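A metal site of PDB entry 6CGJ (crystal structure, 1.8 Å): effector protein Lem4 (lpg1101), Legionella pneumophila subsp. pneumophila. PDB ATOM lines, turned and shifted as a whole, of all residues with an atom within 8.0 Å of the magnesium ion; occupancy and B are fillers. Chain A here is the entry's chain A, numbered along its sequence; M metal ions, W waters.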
ATOM      1  N   LEU A  22     -35.219  18.977  12.222  1.00  0.00           N
ATOM      2  CA  LEU A  22     -34.598  18.887  10.911  1.00  0.00           C
ATOM      3  C   LEU A  22     -33.085  18.904  11.041  1.00  0.00           C
ATOM      4  O   LEU A  22     -32.519  19.817  11.650  1.00  0.00           O
ATOM      5  CB  LEU A  22     -35.030  20.045  10.001  1.00  0.00           C
ATOM      6  CG  LEU A  22     -36.537  20.194   9.774  1.00  0.00           C
ATOM      7  CD1 LEU A  22     -36.818  21.442   8.905  1.00  0.00           C
ATOM      8  CD2 LEU A  22     -37.107  18.927   9.141  1.00  0.00           C
ATOM      9  N   ASP A  23     -32.433  17.909  10.472  1.00  0.00           N
ATOM     10  CA  ASP A  23     -31.028  18.049  10.107  1.00  0.00           C
ATOM     11  C   ASP A  23     -30.884  19.188   9.104  1.00  0.00           C
ATOM     12  O   ASP A  23     -31.828  19.546   8.395  1.00  0.00           O
ATOM     13  CB  ASP A  23     -30.529  16.725   9.532  1.00  0.00           C
ATOM     14  CG  ASP A  23     -29.114  16.823   8.970  1.00  0.00           C
ATOM     15  OD1 ASP A  23     -28.199  17.193   9.737  1.00  0.00           O
ATOM     16  OD2 ASP A  23     -28.926  16.527   7.775  1.00  0.00           O
ATOM     17  N   PHE A  24     -29.666  19.755   9.003  1.00  0.00           N
ATOM     18  CA  PHE A  24     -29.456  20.810   8.028  1.00  0.00           C
ATOM     19  C   PHE A  24     -28.803  20.280   6.751  1.00  0.00           C
ATOM     20  O   PHE A  24     -29.454  20.215   5.703  1.00  0.00           O
ATOM     21  CB  PHE A  24     -28.616  21.946   8.626  1.00  0.00           C
ATOM     22  CG  PHE A  24     -28.492  23.140   7.707  1.00  0.00           C
ATOM     23  CD1 PHE A  24     -29.572  23.987   7.505  1.00  0.00           C
ATOM     24  CD2 PHE A  24     -27.300  23.391   7.050  1.00  0.00           C
ATOM     25  CE1 PHE A  24     -29.458  25.089   6.639  1.00  0.00           C
ATOM     26  CE2 PHE A  24     -27.179  24.484   6.191  1.00  0.00           C
ATOM     27  CZ  PHE A  24     -28.259  25.330   5.989  1.00  0.00           C
ATOM     28  N   ASP A  25     -27.538  19.858   6.819  1.00  0.00           N
ATOM     29  CA  ASP A  25     -26.776  19.532   5.616  1.00  0.00           C
ATOM     30  C   ASP A  25     -27.287  18.251   4.960  1.00  0.00           C
ATOM     31  O   ASP A  25     -27.249  17.178   5.557  1.00  0.00           O
ATOM     32  CB  ASP A  25     -25.292  19.396   5.957  1.00  0.00           C
ATOM     33  CG  ASP A  25     -24.680  20.707   6.410  1.00  0.00           C
ATOM     34  OD1 ASP A  25     -24.356  20.830   7.604  1.00  0.00           O
ATOM     35  OD2 ASP A  25     -24.486  21.593   5.555  1.00  0.00           O
ATOM     36  N   GLY A  26     -27.711  18.356   3.692  1.00  0.00           N
ATOM     37  CA  GLY A  26     -28.226  17.216   2.955  1.00  0.00           C
ATOM     38  C   GLY A  26     -29.677  16.930   3.219  1.00  0.00           C
ATOM     39  O   GLY A  26     -30.256  16.042   2.575  1.00  0.00           O
ATOM     40  N   THR A  27     -30.284  17.609   4.179  1.00  0.00           N
ATOM     41  CA  THR A  27     -31.710  17.510   4.437  1.00  0.00           C
ATOM     42  C   THR A  27     -32.403  18.766   3.945  1.00  0.00           C
ATOM     43  O   THR A  27     -33.195  18.713   3.002  1.00  0.00           O
ATOM     44  CB  THR A  27     -31.964  17.278   5.941  1.00  0.00           C
ATOM     45  OG1 THR A  27     -31.259  16.089   6.359  1.00  0.00           O
ATOM     46  CG2 THR A  27     -33.468  17.110   6.212  1.00  0.00           C
ATOM     47  N   ILE A  28     -32.077  19.925   4.535  1.00  0.00           N
ATOM     48  CA  ILE A  28     -32.534  21.215   4.032  1.00  0.00           C
ATOM     49  C   ILE A  28     -31.748  21.625   2.785  1.00  0.00           C
ATOM     50  O   ILE A  28     -32.309  22.257   1.882  1.00  0.00           O
ATOM     51  CB  ILE A  28     -32.425  22.236   5.173  1.00  0.00           C
ATOM     52  CG1 ILE A  28     -33.490  21.920   6.244  1.00  0.00           C
ATOM     53  CG2 ILE A  28     -32.564  23.666   4.668  1.00  0.00           C
ATOM     54  CD1 ILE A  28     -33.314  22.705   7.537  1.00  0.00           C
ATOM     55  N   THR A  29     -30.466  21.265   2.695  1.00  0.00           N
ATOM     56  CA  THR A  29     -29.660  21.519   1.508  1.00  0.00           C
ATOM     57  C   THR A  29     -29.534  20.245   0.678  1.00  0.00           C
ATOM     58  O   THR A  29     -29.973  19.165   1.075  1.00  0.00           O
ATOM     59  CB  THR A  29     -28.264  22.042   1.883  1.00  0.00           C
ATOM     60  OG1 THR A  29     -27.518  21.006   2.514  1.00  0.00           O
ATOM     61  CG2 THR A  29     -28.351  23.240   2.834  1.00  0.00           C
ATOM     62  N   ALA A  31     -26.560  18.803  -0.148  1.00  0.00           N
ATOM     63  CA  ALA A  31     -25.211  18.261  -0.037  1.00  0.00           C
ATOM     64  C   ALA A  31     -24.944  17.744   1.370  1.00  0.00           C
ATOM     65  O   ALA A  31     -25.095  18.476   2.345  1.00  0.00           O
ATOM     66  CB  ALA A  31     -24.160  19.323  -0.394  1.00  0.00           C
ATOM     67  N   HIS A  32     -24.511  16.482   1.455  1.00  0.00           N
ATOM     68  CA  HIS A  32     -24.208  15.840   2.736  1.00  0.00           C
ATOM     69  C   HIS A  32     -23.199  16.668   3.535  1.00  0.00           C
ATOM     70  O   HIS A  32     -22.294  17.291   2.984  1.00  0.00           O
ATOM     71  CB  HIS A  32     -23.646  14.433   2.487  1.00  0.00           C
ATOM     72  CG  HIS A  32     -23.439  13.621   3.729  1.00  0.00           C
ATOM     73  ND1 HIS A  32     -22.399  13.860   4.607  1.00  0.00           N
ATOM     74  CD2 HIS A  32     -24.121  12.567   4.227  1.00  0.00           C
ATOM     75  CE1 HIS A  32     -22.462  13.001   5.606  1.00  0.00           C
ATOM     76  NE2 HIS A  32     -23.499  12.196   5.402  1.00  0.00           N
ATOM     77  N   GLY A  33     -23.355  16.633   4.859  1.00  0.00           N
ATOM     78  CA  GLY A  33     -22.546  17.461   5.736  1.00  0.00           C
ATOM     79  C   GLY A  33     -21.045  17.267   5.583  1.00  0.00           C
ATOM     80  O   GLY A  33     -20.277  18.209   5.800  1.00  0.00           O
ATOM     81  N   LYS A  34     -20.614  16.060   5.213  1.00  0.00           N
ATOM     82  CA  LYS A  34     -19.179  15.765   5.143  1.00  0.00           C
ATOM     83  C   LYS A  34     -18.492  16.588   4.064  1.00  0.00           C
ATOM     84  O   LYS A  34     -17.331  17.008   4.239  1.00  0.00           O
ATOM     85  CB  LYS A  34     -18.979  14.271   4.876  1.00  0.00           C
ATOM     86  N   ILE A  93     -31.110  20.825  14.027  1.00  0.00           N
ATOM     87  CA  ILE A  93     -30.015  20.263  14.807  1.00  0.00           C
ATOM     88  C   ILE A  93     -28.904  19.881  13.847  1.00  0.00           C
ATOM     89  O   ILE A  93     -29.147  19.151  12.880  1.00  0.00           O
ATOM     90  CB  ILE A  93     -30.472  19.042  15.620  1.00  0.00           C
ATOM     91  CG1 ILE A  93     -31.739  19.361  16.411  1.00  0.00           C
ATOM     92  CG2 ILE A  93     -29.349  18.629  16.579  1.00  0.00           C
ATOM     93  CD1 ILE A  93     -32.197  18.189  17.307  1.00  0.00           C
ATOM     94  N   SER A  94     -27.687  20.330  14.131  1.00  0.00           N
ATOM     95  CA  SER A  94     -26.632  20.291  13.128  1.00  0.00           C
ATOM     96  C   SER A  94     -25.260  20.376  13.792  1.00  0.00           C
ATOM     97  O   SER A  94     -25.083  21.102  14.776  1.00  0.00           O
ATOM     98  CB  SER A  94     -26.820  21.454  12.144  1.00  0.00           C
ATOM     99  OG  SER A  94     -25.775  21.557  11.207  1.00  0.00           O
ATOM    100  N   ARG A  95     -24.284  19.655  13.244  1.00  0.00           N
ATOM    101  CA  ARG A  95     -22.905  19.863  13.678  1.00  0.00           C
ATOM    102  C   ARG A  95     -22.184  20.879  12.805  1.00  0.00           C
ATOM    103  O   ARG A  95     -20.946  20.995  12.886  1.00  0.00           O
ATOM    104  CB  ARG A  95     -22.158  18.529  13.724  1.00  0.00           C
ATOM    105  CG  ARG A  95     -21.955  17.882  12.376  1.00  0.00           C
ATOM    106  CD  ARG A  95     -21.074  16.645  12.492  1.00  0.00           C
ATOM    107  NE  ARG A  95     -21.649  15.645  13.395  1.00  0.00           N
ATOM    108  CZ  ARG A  95     -22.407  14.631  12.995  1.00  0.00           C
ATOM    109  NH1 ARG A  95     -22.690  14.481  11.708  1.00  0.00           N
ATOM    110  NH2 ARG A  95     -22.899  13.773  13.883  1.00  0.00           N
ATOM    111  N   LYS A 132     -26.903  14.712  18.617  1.00  0.00           N
ATOM    112  CA  LYS A 132     -28.308  14.863  18.244  1.00  0.00           C
ATOM    113  C   LYS A 132     -29.241  14.163  19.222  1.00  0.00           C
ATOM    114  O   LYS A 132     -30.357  14.643  19.465  1.00  0.00           O
ATOM    115  CB  LYS A 132     -28.515  14.325  16.831  1.00  0.00           C
ATOM    116  CG  LYS A 132     -28.178  15.383  15.759  1.00  0.00           C
ATOM    117  CD  LYS A 132     -28.368  14.832  14.367  1.00  0.00           C
ATOM    118  CE  LYS A 132     -28.286  15.977  13.338  1.00  0.00           C
ATOM    119  NZ  LYS A 132     -28.040  15.449  11.971  1.00  0.00           N
ATOM    120  N   CYS A 153     -36.562  14.649  10.105  1.00  0.00           N
ATOM    121  CA  CYS A 153     -35.970  14.448   8.785  1.00  0.00           C
ATOM    122  C   CYS A 153     -34.450  14.490   8.857  1.00  0.00           C
ATOM    123  O   CYS A 153     -33.889  15.419   9.451  1.00  0.00           O
ATOM    124  CB  CYS A 153     -36.461  15.510   7.788  1.00  0.00           C
ATOM    125  SG  CYS A 153     -38.254  15.404   7.580  1.00  0.00           S
ATOM    126  N   ASP A 154     -33.795  13.507   8.231  1.00  0.00           N
ATOM    127  CA  ASP A 154     -32.336  13.447   8.238  1.00  0.00           C
ATOM    128  C   ASP A 154     -31.895  12.593   7.064  1.00  0.00           C
ATOM    129  O   ASP A 154     -32.436  11.515   6.835  1.00  0.00           O
ATOM    130  CB  ASP A 154     -31.809  12.862   9.566  1.00  0.00           C
ATOM    131  CG  ASP A 154     -30.398  13.286   9.872  1.00  0.00           C
ATOM    132  OD1 ASP A 154     -29.574  13.222   8.956  1.00  0.00           O
ATOM    133  OD2 ASP A 154     -30.118  13.695  11.016  1.00  0.00           O
ATOM    134  N   ASP A 155     -30.911  13.096   6.308  1.00  0.00           N
ATOM    135  CA  ASP A 155     -30.387  12.319   5.199  1.00  0.00           C
ATOM    136  C   ASP A 155     -29.465  11.195   5.657  1.00  0.00           C
ATOM    137  O   ASP A 155     -29.174  10.278   4.873  1.00  0.00           O
ATOM    138  CB  ASP A 155     -29.640  13.238   4.221  1.00  0.00           C
ATOM    139  CG  ASP A 155     -28.410  13.870   4.833  1.00  0.00           C
ATOM    140  OD1 ASP A 155     -28.514  14.550   5.871  1.00  0.00           O
ATOM    141  OD2 ASP A 155     -27.311  13.689   4.235  1.00  0.00           O
ATOM    142  N   ASP A 156     -29.009  11.236   6.912  1.00  0.00           N
ATOM    143  CA  ASP A 156     -28.100  10.242   7.479  1.00  0.00           C
ATOM    144  C   ASP A 156     -28.887   9.360   8.436  1.00  0.00           C
ATOM    145  O   ASP A 156     -29.423   9.850   9.441  1.00  0.00           O
ATOM    146  CB  ASP A 156     -26.940  10.935   8.204  1.00  0.00           C
ATOM    147  CG  ASP A 156     -25.867   9.960   8.658  1.00  0.00           C
ATOM    148  OD1 ASP A 156     -26.179   9.023   9.421  1.00  0.00           O
ATOM    149  OD2 ASP A 156     -24.700  10.125   8.246  1.00  0.00           O
ATOM    150  N   GLU A 157     -28.965   8.070   8.117  1.00  0.00           N
ATOM    151  CA  GLU A 157     -29.827   7.170   8.887  1.00  0.00           C
ATOM    152  C   GLU A 157     -29.382   7.079  10.337  1.00  0.00           C
ATOM    153  O   GLU A 157     -30.219   7.049  11.249  1.00  0.00           O
ATOM    154  CB  GLU A 157     -29.835   5.779   8.242  1.00  0.00           C
ATOM    155  CG  GLU A 157     -30.921   4.868   8.802  1.00  0.00           C
ATOM    156  CD  GLU A 157     -30.980   3.545   8.065  1.00  0.00           C
ATOM    157  OE1 GLU A 157     -29.975   3.171   7.420  1.00  0.00           O
ATOM    158  OE2 GLU A 157     -32.026   2.869   8.134  1.00  0.00           O
ATOM    159  N   ASP A 159     -27.651   9.414  12.159  1.00  0.00           N
ATOM    160  CA  ASP A 159     -28.052  10.681  12.781  1.00  0.00           C
ATOM    161  C   ASP A 159     -29.543  10.719  13.059  1.00  0.00           C
ATOM    162  O   ASP A 159     -29.981  11.184  14.124  1.00  0.00           O
ATOM    163  CB  ASP A 159     -27.686  11.863  11.881  1.00  0.00           C
ATOM    164  CG  ASP A 159     -26.203  12.212  11.924  1.00  0.00           C
ATOM    165  OD1 ASP A 159     -25.410  11.481  12.538  1.00  0.00           O
ATOM    166  OD2 ASP A 159     -25.836  13.233  11.305  1.00  0.00           O
ATOM    167  N   GLU A 181     -34.344  10.314   3.641  1.00  0.00           N
ATOM    168  CA  GLU A 181     -34.172  10.314   2.197  1.00  0.00           C
ATOM    169  C   GLU A 181     -32.795  10.842   1.850  1.00  0.00           C
ATOM    170  O   GLU A 181     -32.120  11.483   2.660  1.00  0.00           O
ATOM    171  CB  GLU A 181     -35.251  11.176   1.506  1.00  0.00           C
ATOM    172  CG  GLU A 181     -36.694  10.761   1.824  1.00  0.00           C
ATOM    173  CD  GLU A 181     -37.185   9.577   1.001  1.00  0.00           C
ATOM    174  OE1 GLU A 181     -36.457   9.075   0.124  1.00  0.00           O
ATOM    175  OE2 GLU A 181     -38.334   9.127   1.238  1.00  0.00           O
ATOM    176  N   PRO A 183     -30.212  13.418  -0.137  1.00  0.00           N
ATOM    177  CA  PRO A 183     -30.338  14.837  -0.429  1.00  0.00           C
ATOM    178  C   PRO A 183     -31.078  15.072  -1.745  1.00  0.00           C
ATOM    179  O   PRO A 183     -30.853  14.372  -2.738  1.00  0.00           O
ATOM    180  CB  PRO A 183     -28.887  15.313  -0.502  1.00  0.00           C
ATOM    181  CG  PRO A 183     -28.165  14.389   0.425  1.00  0.00           C
ATOM    182  CD  PRO A 183     -28.832  13.051   0.258  1.00  0.00           C
ATOM    183  N   PHE A 186     -36.292  14.534  -0.501  1.00  0.00           N
ATOM    184  CA  PHE A 186     -37.279  14.634   0.562  1.00  0.00           C
ATOM    185  C   PHE A 186     -38.614  15.105  -0.001  1.00  0.00           C
ATOM    186  O   PHE A 186     -38.660  15.979  -0.882  1.00  0.00           O
ATOM    187  CB  PHE A 186     -36.795  15.576   1.661  1.00  0.00           C
ATOM    188  CG  PHE A 186     -35.735  14.971   2.529  1.00  0.00           C
ATOM    189  CD1 PHE A 186     -36.073  14.225   3.641  1.00  0.00           C
ATOM    190  CD2 PHE A 186     -34.391  15.143   2.216  1.00  0.00           C
ATOM    191  CE1 PHE A 186     -35.104  13.665   4.441  1.00  0.00           C
ATOM    192  CE2 PHE A 186     -33.409  14.563   3.015  1.00  0.00           C
ATOM    193  CZ  PHE A 186     -33.765  13.824   4.128  1.00  0.00           C
HETATM  194 MG    MG M   1     -27.244  15.657   6.977  1.00  0.00          MG
HETATM  195  O   HOH W   1     -27.155  14.269   8.523  1.00  0.00           O
HETATM  196  O   HOH W   2     -25.975  16.784   8.181  1.00  0.00           O
HETATM  197  O   HOH W   3     -25.532  14.827   5.963  1.00  0.00           O
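Residues that only touch the magnesium ion: Asp 154 (3.9 Å). Within 4 Å of the magnesium ion: Asp 23, Asp 25, Asp 154 and Asp 155. Along chain A the residues within 4 Å of the magnesium ion span positions 23 to 155.
The side-chain carboxylate (OD1) of Asp 155 binds the magnesium ion, at 2.0 Å. The magnesium ion is bound by the side-chain carboxylate (OD2) of Asp 23, at 2.1 Å. The magnesium ion is bound by water W1, at 2.1 Å. O of Asp 25 is bound to the magnesium ion, 2.1 Å away. Water W2 is bound to the magnesium ion (2.1 Å). Water W3 binds the magnesium ion (2.2 Å).
OD1 of Asp 23 lies within salt-bridge range of NZ of Lys 132 (2.8 Å). The side-chain hydroxyl (OG1) of Thr 27 sits close to the side-chain carboxylate (OD2) of Asp 23, at 2.8 Å. OD1 of Asp 154 lies within hydrogen-bond range of N of Asp 156 (2.9 Å). The backbone NH of Asp 23 sits at hydrogen-bond distance from the backbone carbonyl oxygen of Cys 153 (3.1 Å). The backbone NH of Asp 155 lies within hydrogen-bond range of the side-chain hydroxyl of Thr 27 (3.0 Å). The side-chain carboxylate (OD2) of Asp 154 is in salt-bridge range of the side-chain amino group (NZ) of Lys 132 (2.9 Å).
Water W3 lies within hydrogen-bond range of OD2 of Asp 155 (2.7 Å), N of Gly 33 (3.0 Å) and NE2 of His 32 (3.4 Å).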
